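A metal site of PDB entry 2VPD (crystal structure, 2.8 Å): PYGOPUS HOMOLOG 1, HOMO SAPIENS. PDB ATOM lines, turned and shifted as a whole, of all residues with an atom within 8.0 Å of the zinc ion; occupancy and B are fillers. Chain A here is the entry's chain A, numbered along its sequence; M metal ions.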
ATOM      1  N   TYR A  10      17.373 -33.155  -5.546  1.00  0.00           N
ATOM      2  CA  TYR A  10      16.983 -32.973  -4.134  1.00  0.00           C
ATOM      3  C   TYR A  10      15.754 -32.081  -3.957  1.00  0.00           C
ATOM      4  O   TYR A  10      15.782 -30.903  -4.348  1.00  0.00           O
ATOM      5  CB  TYR A  10      18.156 -32.405  -3.313  1.00  0.00           C
ATOM      6  CG  TYR A  10      19.338 -33.344  -3.158  1.00  0.00           C
ATOM      7  CD1 TYR A  10      19.437 -34.185  -2.043  1.00  0.00           C
ATOM      8  CD2 TYR A  10      20.350 -33.380  -4.126  1.00  0.00           C
ATOM      9  CE1 TYR A  10      20.535 -35.055  -1.887  1.00  0.00           C
ATOM     10  CE2 TYR A  10      21.458 -34.247  -3.980  1.00  0.00           C
ATOM     11  CZ  TYR A  10      21.533 -35.076  -2.868  1.00  0.00           C
ATOM     12  OH  TYR A  10      22.616 -35.930  -2.724  1.00  0.00           O
ATOM     13  N   PRO A  11      14.669 -32.627  -3.369  1.00  0.00           N
ATOM     14  CA  PRO A  11      13.489 -31.799  -3.144  1.00  0.00           C
ATOM     15  C   PRO A  11      13.693 -30.870  -1.940  1.00  0.00           C
ATOM     16  O   PRO A  11      14.235 -31.303  -0.923  1.00  0.00           O
ATOM     17  CB  PRO A  11      12.382 -32.822  -2.872  1.00  0.00           C
ATOM     18  CG  PRO A  11      13.106 -33.983  -2.262  1.00  0.00           C
ATOM     19  CD  PRO A  11      14.479 -34.003  -2.881  1.00  0.00           C
ATOM     20  N   CYS A  12      13.281 -29.612  -2.079  1.00  0.00           N
ATOM     21  CA  CYS A  12      13.366 -28.656  -0.993  1.00  0.00           C
ATOM     22  C   CYS A  12      12.397 -29.047   0.101  1.00  0.00           C
ATOM     23  O   CYS A  12      11.182 -29.090  -0.121  1.00  0.00           O
ATOM     24  CB  CYS A  12      13.053 -27.244  -1.480  1.00  0.00           C
ATOM     25  SG  CYS A  12      12.907 -26.001  -0.168  1.00  0.00           S
ATOM     26  N   GLY A  13      12.927 -29.354   1.277  1.00  0.00           N
ATOM     27  CA  GLY A  13      12.108 -29.759   2.401  1.00  0.00           C
ATOM     28  C   GLY A  13      10.866 -28.899   2.610  1.00  0.00           C
ATOM     29  O   GLY A  13       9.852 -29.391   3.097  1.00  0.00           O
ATOM     30  N   ILE A  14      10.947 -27.620   2.224  1.00  0.00           N
ATOM     31  CA  ILE A  14       9.820 -26.686   2.404  1.00  0.00           C
ATOM     32  C   ILE A  14       8.890 -26.609   1.184  1.00  0.00           C
ATOM     33  O   ILE A  14       7.711 -26.936   1.287  1.00  0.00           O
ATOM     34  CB  ILE A  14      10.306 -25.271   2.832  1.00  0.00           C
ATOM     35  CG1 ILE A  14      10.738 -25.286   4.302  1.00  0.00           C
ATOM     36  CG2 ILE A  14       9.210 -24.236   2.644  1.00  0.00           C
ATOM     37  CD1 ILE A  14      11.265 -23.977   4.821  1.00  0.00           C
ATOM     38  N   CYS A  15       9.432 -26.184   0.044  1.00  0.00           N
ATOM     39  CA  CYS A  15       8.616 -25.934  -1.143  1.00  0.00           C
ATOM     40  C   CYS A  15       8.503 -27.155  -2.059  1.00  0.00           C
ATOM     41  O   CYS A  15       7.624 -27.208  -2.925  1.00  0.00           O
ATOM     42  CB  CYS A  15       9.175 -24.746  -1.918  1.00  0.00           C
ATOM     43  SG  CYS A  15      10.523 -25.184  -3.009  1.00  0.00           S
ATOM     44  N   THR A  16       9.407 -28.113  -1.877  1.00  0.00           N
ATOM     45  CA  THR A  16       9.432 -29.429  -2.577  1.00  0.00           C
ATOM     46  C   THR A  16       9.949 -29.439  -4.025  1.00  0.00           C
ATOM     47  O   THR A  16      10.017 -30.494  -4.643  1.00  0.00           O
ATOM     48  CB  THR A  16       8.071 -30.221  -2.487  1.00  0.00           C
ATOM     49  OG1 THR A  16       7.165 -29.761  -3.495  1.00  0.00           O
ATOM     50  CG2 THR A  16       7.434 -30.116  -1.093  1.00  0.00           C
ATOM     51  N   ASN A  17      10.307 -28.268  -4.549  1.00  0.00           N
ATOM     52  CA  ASN A  17      10.969 -28.189  -5.856  1.00  0.00           C
ATOM     53  C   ASN A  17      12.447 -28.583  -5.768  1.00  0.00           C
ATOM     54  O   ASN A  17      13.016 -28.666  -4.677  1.00  0.00           O
ATOM     55  CB  ASN A  17      10.861 -26.787  -6.442  1.00  0.00           C
ATOM     56  CG  ASN A  17       9.434 -26.284  -6.537  1.00  0.00           C
ATOM     57  OD1 ASN A  17       8.731 -26.203  -5.525  1.00  0.00           O
ATOM     58  ND2 ASN A  17       9.005 -25.929  -7.742  1.00  0.00           N
ATOM     59  N   GLU A  18      13.060 -28.800  -6.934  1.00  0.00           N
ATOM     60  CA  GLU A  18      14.492 -29.098  -7.016  1.00  0.00           C
ATOM     61  C   GLU A  18      15.353 -28.003  -6.393  1.00  0.00           C
ATOM     62  O   GLU A  18      14.983 -26.826  -6.403  1.00  0.00           O
ATOM     63  CB  GLU A  18      14.925 -29.281  -8.476  1.00  0.00           C
ATOM     64  CG  GLU A  18      15.136 -30.717  -8.916  1.00  0.00           C
ATOM     65  CD  GLU A  18      15.349 -30.825 -10.433  1.00  0.00           C
ATOM     66  OE1 GLU A  18      16.418 -31.339 -10.859  1.00  0.00           O
ATOM     67  OE2 GLU A  18      14.461 -30.379 -11.197  1.00  0.00           O
ATOM     68  N   VAL A  19      16.502 -28.424  -5.867  1.00  0.00           N
ATOM     69  CA  VAL A  19      17.500 -27.534  -5.301  1.00  0.00           C
ATOM     70  C   VAL A  19      18.746 -27.556  -6.208  1.00  0.00           C
ATOM     71  O   VAL A  19      19.629 -28.405  -6.035  1.00  0.00           O
ATOM     72  CB  VAL A  19      17.850 -27.963  -3.843  1.00  0.00           C
ATOM     73  CG1 VAL A  19      18.846 -27.005  -3.212  1.00  0.00           C
ATOM     74  CG2 VAL A  19      16.585 -28.047  -3.000  1.00  0.00           C
ATOM     75  N   GLN A  23      21.573 -22.088  -6.924  1.00  0.00           N
ATOM     76  CA  GLN A  23      20.782 -21.482  -5.847  1.00  0.00           C
ATOM     77  C   GLN A  23      21.477 -21.491  -4.484  1.00  0.00           C
ATOM     78  O   GLN A  23      22.499 -22.150  -4.299  1.00  0.00           O
ATOM     79  CB  GLN A  23      19.449 -22.199  -5.712  1.00  0.00           C
ATOM     80  CG  GLN A  23      18.535 -22.007  -6.879  1.00  0.00           C
ATOM     81  CD  GLN A  23      17.408 -23.010  -6.881  1.00  0.00           C
ATOM     82  OE1 GLN A  23      17.624 -24.210  -6.737  1.00  0.00           O
ATOM     83  NE2 GLN A  23      16.188 -22.525  -7.054  1.00  0.00           N
ATOM     84  N   ASP A  24      20.896 -20.740  -3.548  1.00  0.00           N
ATOM     85  CA  ASP A  24      21.326 -20.774  -2.157  1.00  0.00           C
ATOM     86  C   ASP A  24      20.592 -21.897  -1.466  1.00  0.00           C
ATOM     87  O   ASP A  24      19.357 -21.959  -1.496  1.00  0.00           O
ATOM     88  CB  ASP A  24      21.003 -19.442  -1.454  1.00  0.00           C
ATOM     89  CG  ASP A  24      22.068 -18.386  -1.680  1.00  0.00           C
ATOM     90  OD1 ASP A  24      22.918 -18.548  -2.587  1.00  0.00           O
ATOM     91  OD2 ASP A  24      22.052 -17.378  -0.945  1.00  0.00           O
ATOM     92  N   TRP A  35      17.810 -30.927   2.410  1.00  0.00           N
ATOM     93  CA  TRP A  35      18.251 -29.648   1.862  1.00  0.00           C
ATOM     94  C   TRP A  35      17.046 -28.732   1.658  1.00  0.00           C
ATOM     95  O   TRP A  35      15.931 -29.199   1.394  1.00  0.00           O
ATOM     96  CB  TRP A  35      18.997 -29.840   0.541  1.00  0.00           C
ATOM     97  CG  TRP A  35      20.366 -30.436   0.729  1.00  0.00           C
ATOM     98  CD1 TRP A  35      20.674 -31.761   0.818  1.00  0.00           C
ATOM     99  CD2 TRP A  35      21.609 -29.723   0.850  1.00  0.00           C
ATOM    100  NE1 TRP A  35      22.026 -31.922   0.992  1.00  0.00           N
ATOM    101  CE2 TRP A  35      22.622 -30.691   1.009  1.00  0.00           C
ATOM    102  CE3 TRP A  35      21.959 -28.370   0.834  1.00  0.00           C
ATOM    103  CZ2 TRP A  35      23.985 -30.338   1.154  1.00  0.00           C
ATOM    104  CZ3 TRP A  35      23.303 -28.023   0.979  1.00  0.00           C
ATOM    105  CH2 TRP A  35      24.300 -29.006   1.148  1.00  0.00           C
ATOM    106  N   PHE A  36      17.279 -27.420   1.809  1.00  0.00           N
ATOM    107  CA  PHE A  36      16.223 -26.412   1.646  1.00  0.00           C
ATOM    108  C   PHE A  36      16.796 -25.206   0.910  1.00  0.00           C
ATOM    109  O   PHE A  36      17.981 -24.919   1.030  1.00  0.00           O
ATOM    110  CB  PHE A  36      15.735 -25.939   3.019  1.00  0.00           C
ATOM    111  CG  PHE A  36      15.237 -27.033   3.922  1.00  0.00           C
ATOM    112  CD1 PHE A  36      13.866 -27.220   4.115  1.00  0.00           C
ATOM    113  CD2 PHE A  36      16.127 -27.854   4.605  1.00  0.00           C
ATOM    114  CE1 PHE A  36      13.393 -28.218   4.961  1.00  0.00           C
ATOM    115  CE2 PHE A  36      15.667 -28.858   5.451  1.00  0.00           C
ATOM    116  CZ  PHE A  36      14.294 -29.038   5.624  1.00  0.00           C
ATOM    117  N   HIS A  37      15.942 -24.496   0.157  1.00  0.00           N
ATOM    118  CA  HIS A  37      16.297 -23.178  -0.358  1.00  0.00           C
ATOM    119  C   HIS A  37      16.428 -22.211   0.809  1.00  0.00           C
ATOM    120  O   HIS A  37      15.571 -22.198   1.707  1.00  0.00           O
ATOM    121  CB  HIS A  37      15.241 -22.644  -1.329  1.00  0.00           C
ATOM    122  CG  HIS A  37      15.053 -23.486  -2.540  1.00  0.00           C
ATOM    123  ND1 HIS A  37      13.911 -24.210  -2.775  1.00  0.00           N
ATOM    124  CD2 HIS A  37      15.865 -23.716  -3.604  1.00  0.00           C
ATOM    125  CE1 HIS A  37      14.027 -24.859  -3.924  1.00  0.00           C
ATOM    126  NE2 HIS A  37      15.200 -24.573  -4.446  1.00  0.00           N
ATOM    127  N   ARG A  38      17.487 -21.398   0.802  1.00  0.00           N
ATOM    128  CA  ARG A  38      17.700 -20.378   1.819  1.00  0.00           C
ATOM    129  C   ARG A  38      16.518 -19.422   1.854  1.00  0.00           C
ATOM    130  O   ARG A  38      16.077 -19.004   2.923  1.00  0.00           O
ATOM    131  CB  ARG A  38      18.983 -19.586   1.534  1.00  0.00           C
ATOM    132  CG  ARG A  38      19.268 -18.492   2.549  1.00  0.00           C
ATOM    133  CD  ARG A  38      20.118 -17.386   1.986  1.00  0.00           C
ATOM    134  NE  ARG A  38      19.608 -16.862   0.714  1.00  0.00           N
ATOM    135  CZ  ARG A  38      18.742 -15.865   0.601  1.00  0.00           C
ATOM    136  NH1 ARG A  38      18.245 -15.265   1.673  1.00  0.00           N
ATOM    137  NH2 ARG A  38      18.354 -15.476  -0.605  1.00  0.00           N
ATOM    138  N   ILE A  39      16.021 -19.085   0.666  1.00  0.00           N
ATOM    139  CA  ILE A  39      14.837 -18.242   0.508  1.00  0.00           C
ATOM    140  C   ILE A  39      13.613 -18.860   1.225  1.00  0.00           C
ATOM    141  O   ILE A  39      12.956 -18.187   2.022  1.00  0.00           O
ATOM    142  CB  ILE A  39      14.539 -17.979  -0.994  1.00  0.00           C
ATOM    143  CG1 ILE A  39      15.729 -17.260  -1.650  1.00  0.00           C
ATOM    144  CG2 ILE A  39      13.259 -17.166  -1.165  1.00  0.00           C
ATOM    145  CD1 ILE A  39      16.006 -17.688  -3.088  1.00  0.00           C
ATOM    146  N   CYS A  40      13.365 -20.145   0.960  1.00  0.00           N
ATOM    147  CA  CYS A  40      12.226 -20.855   1.547  1.00  0.00           C
ATOM    148  C   CYS A  40      12.205 -20.897   3.076  1.00  0.00           C
ATOM    149  O   CYS A  40      11.140 -20.827   3.687  1.00  0.00           O
ATOM    150  CB  CYS A  40      12.152 -22.271   1.000  1.00  0.00           C
ATOM    151  SG  CYS A  40      11.559 -22.293  -0.677  1.00  0.00           S
ATOM    152  N   THR A  41      13.392 -21.005   3.689  1.00  0.00           N
ATOM    153  CA  THR A  41      13.523 -21.028   5.154  1.00  0.00           C
ATOM    154  C   THR A  41      13.226 -19.673   5.797  1.00  0.00           C
ATOM    155  O   THR A  41      12.938 -19.596   6.991  1.00  0.00           O
ATOM    156  CB  THR A  41      14.958 -21.414   5.571  1.00  0.00           C
ATOM    157  OG1 THR A  41      15.866 -20.379   5.177  1.00  0.00           O
ATOM    158  CG2 THR A  41      15.388 -22.728   4.942  1.00  0.00           C
HETATM  159 ZN    ZN M   1      12.192 -24.386  -1.556  1.00  0.00          ZN
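A ring nitrogen (NE2) of His 37 sits at hydrogen-bond distance from the backbone carbonyl oxygen of Glu 18, 3.0 Å away. NE2 of His 37 lies within hydrogen-bond range of OE1 of Gln 23, 3.4 Å away. N of Ile 14 lies close to SG of Cys 12 (3.5 Å). The backbone NH of Cys 12 sits at hydrogen-bond distance from the backbone carbonyl oxygen of Asn 17 (2.8 Å). O of Cys 15 lies close to OD1 of Asn 17, at 3.0 Å.
ND1 of His 37 binds the zinc ion, at 2.1 Å. SG of Cys 12 is bound to the zinc ion, 2.2 Å away. The side-chain sulfur (SG) of Cys 15 binds the zinc ion (2.4 Å). The zinc ion is bound by SG of Cys 40, 2.4 Å away. The zinc ion has four donor atoms within binding distance.
Of the 19 residues printed, 4 come within 4 Å of the zinc ion. The nearest printed residue that does not touch the zinc ion is Thr 16 (4.7 Å).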
